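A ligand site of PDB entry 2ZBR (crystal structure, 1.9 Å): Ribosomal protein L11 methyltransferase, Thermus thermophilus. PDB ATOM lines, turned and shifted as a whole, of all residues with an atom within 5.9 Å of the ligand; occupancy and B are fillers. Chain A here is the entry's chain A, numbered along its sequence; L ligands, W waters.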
ATOM      1  N   GLY A 102     -35.681 -15.649   3.309  1.00  0.00           N
ATOM      2  CA  GLY A 102     -35.654 -15.397   1.874  1.00  0.00           C
ATOM      3  C   GLY A 102     -35.245 -13.993   1.476  1.00  0.00           C
ATOM      4  O   GLY A 102     -35.694 -13.468   0.451  1.00  0.00           O
ATOM      5  N   THR A 106     -28.785 -15.571  -2.448  1.00  0.00           N
ATOM      6  CA  THR A 106     -28.548 -17.006  -2.658  1.00  0.00           C
ATOM      7  C   THR A 106     -29.812 -17.845  -2.510  1.00  0.00           C
ATOM      8  O   THR A 106     -30.021 -18.795  -3.264  1.00  0.00           O
ATOM      9  CB  THR A 106     -27.490 -17.515  -1.703  1.00  0.00           C
ATOM     10  OG1 THR A 106     -27.880 -17.249  -0.356  1.00  0.00           O
ATOM     11  CG2 THR A 106     -26.107 -16.787  -1.983  1.00  0.00           C
ATOM     12  N   THR A 107     -30.629 -17.488  -1.527  1.00  0.00           N
ATOM     13  CA  THR A 107     -31.903 -18.169  -1.302  1.00  0.00           C
ATOM     14  C   THR A 107     -32.787 -17.959  -2.516  1.00  0.00           C
ATOM     15  O   THR A 107     -33.485 -18.891  -2.992  1.00  0.00           O
ATOM     16  CB  THR A 107     -32.602 -17.601  -0.072  1.00  0.00           C
ATOM     17  OG1 THR A 107     -31.806 -17.884   1.074  1.00  0.00           O
ATOM     18  CG2 THR A 107     -33.990 -18.271   0.133  1.00  0.00           C
ATOM     19  N   ALA A 110     -31.585 -19.958  -5.427  1.00  0.00           N
ATOM     20  CA  ALA A 110     -31.892 -21.347  -5.158  1.00  0.00           C
ATOM     21  C   ALA A 110     -33.356 -21.688  -5.439  1.00  0.00           C
ATOM     22  O   ALA A 110     -33.626 -22.738  -5.988  1.00  0.00           O
ATOM     23  CB  ALA A 110     -31.498 -21.703  -3.725  1.00  0.00           C
ATOM     24  N   ASP A 126     -32.193 -31.012   0.950  1.00  0.00           N
ATOM     25  CA  ASP A 126     -31.901 -29.592   1.128  1.00  0.00           C
ATOM     26  C   ASP A 126     -30.793 -29.650   2.229  1.00  0.00           C
ATOM     27  O   ASP A 126     -31.065 -29.850   3.404  1.00  0.00           O
ATOM     28  CB  ASP A 126     -33.120 -28.845   1.661  1.00  0.00           C
ATOM     29  CG  ASP A 126     -32.823 -27.387   1.976  1.00  0.00           C
ATOM     30  OD1 ASP A 126     -31.710 -26.910   1.611  1.00  0.00           O
ATOM     31  OD2 ASP A 126     -33.682 -26.735   2.583  1.00  0.00           O
ATOM     32  N   LEU A 127     -29.542 -29.547   1.795  1.00  0.00           N
ATOM     33  CA  LEU A 127     -28.408 -29.646   2.702  1.00  0.00           C
ATOM     34  C   LEU A 127     -28.078 -28.303   3.320  1.00  0.00           C
ATOM     35  O   LEU A 127     -27.621 -27.416   2.635  1.00  0.00           O
ATOM     36  CB  LEU A 127     -27.217 -30.190   1.926  1.00  0.00           C
ATOM     37  CG  LEU A 127     -25.940 -30.412   2.732  1.00  0.00           C
ATOM     38  CD1 LEU A 127     -26.154 -31.493   3.772  1.00  0.00           C
ATOM     39  CD2 LEU A 127     -24.770 -30.749   1.725  1.00  0.00           C
ATOM     40  N   GLY A 128     -28.262 -28.201   4.648  1.00  0.00           N
ATOM     41  CA  GLY A 128     -28.010 -26.960   5.369  1.00  0.00           C
ATOM     42  C   GLY A 128     -29.311 -26.189   5.250  1.00  0.00           C
ATOM     43  O   GLY A 128     -29.366 -25.004   4.842  1.00  0.00           O
ATOM     44  N   THR A 129     -30.392 -26.874   5.624  1.00  0.00           N
ATOM     45  CA  THR A 129     -31.774 -26.344   5.480  1.00  0.00           C
ATOM     46  C   THR A 129     -32.109 -25.060   6.230  1.00  0.00           C
ATOM     47  O   THR A 129     -32.933 -24.288   5.773  1.00  0.00           O
ATOM     48  CB  THR A 129     -32.809 -27.485   5.828  1.00  0.00           C
ATOM     49  OG1 THR A 129     -34.083 -27.174   5.235  1.00  0.00           O
ATOM     50  CG2 THR A 129     -32.962 -27.628   7.374  1.00  0.00           C
ATOM     51  N   GLY A 130     -31.470 -24.795   7.383  1.00  0.00           N
ATOM     52  CA  GLY A 130     -31.788 -23.556   8.089  1.00  0.00           C
ATOM     53  C   GLY A 130     -33.267 -23.375   8.452  1.00  0.00           C
ATOM     54  O   GLY A 130     -33.844 -24.198   9.132  1.00  0.00           O
ATOM     55  N   SER A 131     -33.851 -22.281   7.973  1.00  0.00           N
ATOM     56  CA  SER A 131     -35.258 -21.942   8.169  1.00  0.00           C
ATOM     57  C   SER A 131     -36.201 -23.006   7.513  1.00  0.00           C
ATOM     58  O   SER A 131     -37.412 -22.976   7.774  1.00  0.00           O
ATOM     59  CB  SER A 131     -35.586 -20.617   7.478  1.00  0.00           C
ATOM     60  OG  SER A 131     -35.525 -20.784   6.050  1.00  0.00           O
ATOM     61  N   GLY A 132     -35.627 -23.873   6.662  1.00  0.00           N
ATOM     62  CA  GLY A 132     -36.368 -24.909   5.918  1.00  0.00           C
ATOM     63  C   GLY A 132     -37.017 -24.376   4.631  1.00  0.00           C
ATOM     64  O   GLY A 132     -37.743 -25.096   3.954  1.00  0.00           O
ATOM     65  N   VAL A 133     -36.720 -23.119   4.256  1.00  0.00           N
ATOM     66  CA  VAL A 133     -37.347 -22.504   3.082  1.00  0.00           C
ATOM     67  C   VAL A 133     -37.224 -23.299   1.791  1.00  0.00           C
ATOM     68  O   VAL A 133     -38.214 -23.406   1.037  1.00  0.00           O
ATOM     69  CB  VAL A 133     -36.812 -21.058   2.832  1.00  0.00           C
ATOM     70  CG1 VAL A 133     -35.256 -21.057   2.487  1.00  0.00           C
ATOM     71  CG2 VAL A 133     -37.583 -20.425   1.656  1.00  0.00           C
ATOM     72  N   LEU A 134     -36.042 -23.868   1.527  1.00  0.00           N
ATOM     73  CA  LEU A 134     -35.869 -24.596   0.279  1.00  0.00           C
ATOM     74  C   LEU A 134     -36.649 -25.924   0.286  1.00  0.00           C
ATOM     75  O   LEU A 134     -37.277 -26.283  -0.714  1.00  0.00           O
ATOM     76  CB  LEU A 134     -34.383 -24.797  -0.066  1.00  0.00           C
ATOM     77  CG  LEU A 134     -33.601 -23.438  -0.191  1.00  0.00           C
ATOM     78  CD1 LEU A 134     -32.128 -23.751  -0.458  1.00  0.00           C
ATOM     79  CD2 LEU A 134     -34.148 -22.517  -1.322  1.00  0.00           C
ATOM     80  N   VAL A 148     -31.682 -31.246   6.047  1.00  0.00           N
ATOM     81  CA  VAL A 148     -30.772 -31.548   7.162  1.00  0.00           C
ATOM     82  C   VAL A 148     -29.935 -30.295   7.536  1.00  0.00           C
ATOM     83  O   VAL A 148     -29.675 -29.395   6.703  1.00  0.00           O
ATOM     84  CB  VAL A 148     -29.811 -32.705   6.841  1.00  0.00           C
ATOM     85  CG1 VAL A 148     -30.594 -33.948   6.373  1.00  0.00           C
ATOM     86  CG2 VAL A 148     -28.766 -32.253   5.820  1.00  0.00           C
ATOM     87  N   ASP A 149     -29.597 -30.188   8.814  1.00  0.00           N
ATOM     88  CA  ASP A 149     -28.758 -29.071   9.244  1.00  0.00           C
ATOM     89  C   ASP A 149     -27.885 -29.563  10.404  1.00  0.00           C
ATOM     90  O   ASP A 149     -28.347 -30.350  11.242  1.00  0.00           O
ATOM     91  CB  ASP A 149     -29.554 -27.887   9.725  1.00  0.00           C
ATOM     92  CG  ASP A 149     -28.796 -26.583   9.571  1.00  0.00           C
ATOM     93  OD1 ASP A 149     -29.168 -25.784   8.716  1.00  0.00           O
ATOM     94  OD2 ASP A 149     -27.797 -26.368  10.288  1.00  0.00           O
ATOM     95  N   ILE A 150     -26.634 -29.122  10.433  1.00  0.00           N
ATOM     96  CA  ILE A 150     -25.761 -29.555  11.550  1.00  0.00           C
ATOM     97  C   ILE A 150     -26.080 -28.848  12.863  1.00  0.00           C
ATOM     98  O   ILE A 150     -25.679 -29.289  13.933  1.00  0.00           O
ATOM     99  CB  ILE A 150     -24.300 -29.366  11.227  1.00  0.00           C
ATOM    100  CG1 ILE A 150     -24.005 -27.920  10.852  1.00  0.00           C
ATOM    101  CG2 ILE A 150     -23.893 -30.360  10.183  1.00  0.00           C
ATOM    102  CD1 ILE A 150     -22.494 -27.639  10.868  1.00  0.00           C
ATOM    103  N   ASP A 151     -26.849 -27.770  12.769  1.00  0.00           N
ATOM    104  CA  ASP A 151     -27.241 -26.998  13.910  1.00  0.00           C
ATOM    105  C   ASP A 151     -28.653 -27.415  14.344  1.00  0.00           C
ATOM    106  O   ASP A 151     -29.656 -26.970  13.752  1.00  0.00           O
ATOM    107  CB  ASP A 151     -27.221 -25.500  13.556  1.00  0.00           C
ATOM    108  CG  ASP A 151     -27.649 -24.613  14.707  1.00  0.00           C
ATOM    109  OD1 ASP A 151     -27.964 -25.175  15.785  1.00  0.00           O
ATOM    110  OD2 ASP A 151     -27.696 -23.362  14.550  1.00  0.00           O
ATOM    111  N   VAL A 154     -32.003 -24.983  14.629  1.00  0.00           N
ATOM    112  CA  VAL A 154     -32.843 -24.470  13.555  1.00  0.00           C
ATOM    113  C   VAL A 154     -33.996 -25.414  13.236  1.00  0.00           C
ATOM    114  O   VAL A 154     -34.977 -24.991  12.644  1.00  0.00           O
ATOM    115  CB  VAL A 154     -32.063 -24.231  12.232  1.00  0.00           C
ATOM    116  CG1 VAL A 154     -30.817 -23.350  12.512  1.00  0.00           C
ATOM    117  CG2 VAL A 154     -31.680 -25.553  11.584  1.00  0.00           C
ATOM    118  N   GLY A 174     -27.921 -33.012  11.214  1.00  0.00           N
ATOM    119  CA  GLY A 174     -26.791 -33.698  10.629  1.00  0.00           C
ATOM    120  C   GLY A 174     -26.425 -33.096   9.317  1.00  0.00           C
ATOM    121  O   GLY A 174     -26.821 -31.973   8.981  1.00  0.00           O
ATOM    122  N   SER A 175     -25.661 -33.852   8.557  1.00  0.00           N
ATOM    123  CA  SER A 175     -25.244 -33.380   7.245  1.00  0.00           C
ATOM    124  C   SER A 175     -25.494 -34.456   6.210  1.00  0.00           C
ATOM    125  O   SER A 175     -26.363 -35.301   6.365  1.00  0.00           O
ATOM    126  CB  SER A 175     -23.761 -32.990   7.250  1.00  0.00           C
ATOM    127  OG  SER A 175     -23.385 -32.387   6.010  1.00  0.00           O
ATOM    128  N   LEU A 176     -24.690 -34.402   5.172  1.00  0.00           N
ATOM    129  CA  LEU A 176     -24.776 -35.336   4.077  1.00  0.00           C
ATOM    130  C   LEU A 176     -24.792 -36.791   4.488  1.00  0.00           C
ATOM    131  O   LEU A 176     -25.658 -37.551   4.055  1.00  0.00           O
ATOM    132  CB  LEU A 176     -23.634 -35.029   3.110  1.00  0.00           C
ATOM    133  CG  LEU A 176     -23.794 -35.554   1.701  1.00  0.00           C
ATOM    134  CD1 LEU A 176     -25.134 -35.100   1.158  1.00  0.00           C
ATOM    135  CD2 LEU A 176     -22.658 -35.033   0.828  1.00  0.00           C
ATOM    136  N   ASN A 191     -27.136 -24.519  -0.185  1.00  0.00           N
ATOM    137  CA  ASN A 191     -26.755 -23.117  -0.092  1.00  0.00           C
ATOM    138  C   ASN A 191     -25.684 -23.082   1.026  1.00  0.00           C
ATOM    139  O   ASN A 191     -26.008 -22.951   2.223  1.00  0.00           O
ATOM    140  CB  ASN A 191     -27.961 -22.251   0.264  1.00  0.00           C
ATOM    141  CG  ASN A 191     -27.635 -20.767   0.231  1.00  0.00           C
ATOM    142  OD1 ASN A 191     -26.482 -20.392   0.010  1.00  0.00           O
ATOM    143  ND2 ASN A 191     -28.636 -19.924   0.421  1.00  0.00           N
ATOM    144  N   LEU A 192     -24.422 -23.268   0.632  1.00  0.00           N
ATOM    145  CA  LEU A 192     -23.324 -23.332   1.590  1.00  0.00           C
ATOM    146  C   LEU A 192     -22.260 -22.308   1.201  1.00  0.00           C
ATOM    147  O   LEU A 192     -22.523 -21.101   1.282  1.00  0.00           O
ATOM    148  CB  LEU A 192     -22.806 -24.787   1.596  1.00  0.00           C
ATOM    149  CG  LEU A 192     -23.879 -25.799   2.076  1.00  0.00           C
ATOM    150  CD1 LEU A 192     -23.444 -27.254   1.812  1.00  0.00           C
ATOM    151  CD2 LEU A 192     -24.213 -25.604   3.583  1.00  0.00           C
ATOM    152  N   TYR A 193     -21.076 -22.767   0.798  1.00  0.00           N
ATOM    153  CA  TYR A 193     -20.027 -21.845   0.316  1.00  0.00           C
ATOM    154  C   TYR A 193     -19.094 -22.654  -0.575  1.00  0.00           C
ATOM    155  O   TYR A 193     -18.996 -23.867  -0.430  1.00  0.00           O
ATOM    156  CB  TYR A 193     -19.326 -21.113   1.487  1.00  0.00           C
ATOM    157  CG  TYR A 193     -18.653 -21.996   2.483  1.00  0.00           C
ATOM    158  CD1 TYR A 193     -17.317 -22.361   2.318  1.00  0.00           C
ATOM    159  CD2 TYR A 193     -19.339 -22.476   3.586  1.00  0.00           C
ATOM    160  CE1 TYR A 193     -16.671 -23.184   3.228  1.00  0.00           C
ATOM    161  CE2 TYR A 193     -18.709 -23.297   4.515  1.00  0.00           C
ATOM    162  CZ  TYR A 193     -17.378 -23.641   4.321  1.00  0.00           C
ATOM    163  OH  TYR A 193     -16.734 -24.422   5.255  1.00  0.00           O
ATOM    164  N   LEU A 196     -16.653 -25.493   0.674  1.00  0.00           N
ATOM    165  CA  LEU A 196     -17.324 -26.656   1.216  1.00  0.00           C
ATOM    166  C   LEU A 196     -17.886 -27.521   0.073  1.00  0.00           C
ATOM    167  O   LEU A 196     -17.796 -28.777   0.112  1.00  0.00           O
ATOM    168  CB  LEU A 196     -18.436 -26.243   2.186  1.00  0.00           C
ATOM    169  CG  LEU A 196     -19.192 -27.390   2.864  1.00  0.00           C
ATOM    170  CD1 LEU A 196     -18.240 -28.489   3.306  1.00  0.00           C
ATOM    171  CD2 LEU A 196     -19.982 -26.854   4.061  1.00  0.00           C
ATOM    172  N   LEU A 200     -17.109 -31.403  -0.867  1.00  0.00           N
ATOM    173  CA  LEU A 200     -18.171 -32.409  -0.921  1.00  0.00           C
ATOM    174  C   LEU A 200     -18.524 -32.987  -2.294  1.00  0.00           C
ATOM    175  O   LEU A 200     -19.256 -33.973  -2.365  1.00  0.00           O
ATOM    176  CB  LEU A 200     -19.456 -31.859  -0.285  1.00  0.00           C
ATOM    177  CG  LEU A 200     -19.388 -31.416   1.177  1.00  0.00           C
ATOM    178  CD1 LEU A 200     -20.681 -30.718   1.536  1.00  0.00           C
ATOM    179  CD2 LEU A 200     -19.139 -32.650   2.093  1.00  0.00           C
ATOM    180  N   THR A 217     -25.233 -23.174  -4.258  1.00  0.00           N
ATOM    181  CA  THR A 217     -25.117 -21.735  -4.165  1.00  0.00           C
ATOM    182  C   THR A 217     -24.410 -21.334  -2.859  1.00  0.00           C
ATOM    183  O   THR A 217     -23.875 -22.209  -2.168  1.00  0.00           O
ATOM    184  CB  THR A 217     -26.488 -21.028  -4.359  1.00  0.00           C
ATOM    185  OG1 THR A 217     -26.274 -19.620  -4.594  1.00  0.00           O
ATOM    186  CG2 THR A 217     -27.412 -21.274  -3.172  1.00  0.00           C
HETATM  187  N1  LIG L   1     -31.017 -23.338   2.890  1.00  0.00           N
HETATM  188  C1  LIG L   1     -31.314 -22.050   3.522  1.00  0.00           C
HETATM  189  C2  LIG L   1     -31.331 -20.949   2.462  1.00  0.00           C
HETATM  190  O1  LIG L   1     -31.047 -21.190   1.290  1.00  0.00           O
HETATM  191  O2  LIG L   1     -31.626 -19.796   2.776  1.00  0.00           O
HETATM  192  C3  LIG L   1     -30.297 -21.739   4.626  1.00  0.00           C
HETATM  193  C4  LIG L   1     -28.845 -21.904   4.171  1.00  0.00           C
HETATM  194  C5  LIG L   1     -27.834 -21.368   5.188  1.00  0.00           C
HETATM  195  N2  LIG L   1     -27.196 -20.174   4.616  1.00  0.00           N
HETATM  196  C6  LIG L   1     -26.738 -22.405   5.439  1.00  0.00           C
HETATM  197  C7  LIG L   1     -27.137 -23.455   6.486  1.00  0.00           C
HETATM  198  O3  LIG L   1     -26.221 -24.557   6.358  1.00  0.00           O
HETATM  199  C8  LIG L   1     -27.022 -22.966   7.937  1.00  0.00           C
HETATM  200  O4  LIG L   1     -28.242 -23.216   8.640  1.00  0.00           O
HETATM  201  C9  LIG L   1     -25.883 -23.802   8.518  1.00  0.00           C
HETATM  202  O5  LIG L   1     -26.129 -24.136   9.882  1.00  0.00           O
HETATM  203  C10 LIG L   1     -26.012 -25.076   7.685  1.00  0.00           C
HETATM  204  N3  LIG L   1     -24.747 -25.852   7.608  1.00  0.00           N
HETATM  205  C11 LIG L   1     -23.528 -25.337   7.470  1.00  0.00           C
HETATM  206  N4  LIG L   1     -22.671 -26.312   7.169  1.00  0.00           N
HETATM  207  C12 LIG L   1     -23.353 -27.454   7.126  1.00  0.00           C
HETATM  208  C13 LIG L   1     -23.009 -28.763   6.840  1.00  0.00           C
HETATM  209  N5  LIG L   1     -21.733 -29.099   6.611  1.00  0.00           N
HETATM  210  N6  LIG L   1     -24.006 -29.741   6.856  1.00  0.00           N
HETATM  211  C14 LIG L   1     -25.329 -29.379   7.163  1.00  0.00           C
HETATM  212  N7  LIG L   1     -25.623 -28.121   7.429  1.00  0.00           N
HETATM  213  C15 LIG L   1     -24.685 -27.162   7.415  1.00  0.00           C
HETATM  214  O   HOH W   1     -33.567 -24.292   3.224  1.00  0.00           O
HETATM  215  O   HOH W   2     -29.119 -18.256   3.950  1.00  0.00           O
HETATM  216  O   HOH W   3     -29.464 -25.363   1.527  1.00  0.00           O
HETATM  217  O   HOH W   4     -32.540 -20.053   6.450  1.00  0.00           O
HETATM  218  O   HOH W   5     -20.263 -31.949   6.300  1.00  0.00           O
HETATM  219  O   HOH W   6     -26.941 -22.570  11.760  1.00  0.00           O
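Water W6 bridges O5 of the ligand (2.6 Å) and OD2 of Asp 151 (3.0 Å). Water W1 lies within hydrogen-bond range of OD2 of Asp 126, O of Thr 129, N1 of the ligand and N of Leu 134. Water W5 lies within hydrogen-bond range of the side-chain hydroxyl of Ser 175 and a nitrogen (N5) of the ligand.
ND2 of Asn 191 sits at hydrogen-bond distance from O1 of the ligand (2.9 Å). N1 of the ligand lies within salt-bridge range of OD1 of Asp 126 (3.9 Å). The backbone NH of Ile 150 is in hydrogen-bond range of a nitrogen (N7) of the ligand, 3.3 Å away. OG of Ser 175 is in hydrogen-bond range of N6 of the ligand. A nitrogen (N1) of the ligand sits at hydrogen-bond distance from the backbone carbonyl oxygen (O) of Gly 128, at 3.1 Å. OG1 of Thr 107 sits at hydrogen-bond distance from O2 of the ligand (2.6 Å). The side-chain carboxylate of Asp 149 lies within hydrogen-bond range of an oxygen (O4) of the ligand (2.7 Å).
Residues that only touch the ligand: Leu 134 (3.3 Å), Gly 174 (3.5 Å), Thr 129 (3.6 Å), Leu 192 (3.6 Å), Gly 130 (3.6 Å), Leu 196 (3.8 Å) and Val 133 (3.9 Å). Hydrophobic or aromatic side chains that line the ligand: Val 133, Leu 134, Ile 150, Leu 192 and Leu 196.
N of Gly 130 is in hydrogen-bond range of OD1 of Asp 149. O of Asp 149 lies within hydrogen-bond range of N of Gly 174, 2.7 Å away. ND2 of Asn 191 is in hydrogen-bond range of OG1 of Thr 106, 2.9 Å away. The side-chain hydroxyl (OG) of Ser 131 sits at hydrogen-bond distance from the backbone NH (N) of Val 133. The backbone NH of Thr 129 lies within hydrogen-bond range of the backbone carbonyl oxygen of Val 148, 2.8 Å away. N of Ile 150 lies within hydrogen-bond range of O of Gly 174 (3.2 Å). The backbone carbonyl oxygen of Asp 126 is in hydrogen-bond range of the backbone NH of Val 148, 3.1 Å away. The side-chain carboxylate (OD1) of Asp 149 is in hydrogen-bond range of the backbone NH (N) of Thr 129 (3.5 Å).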
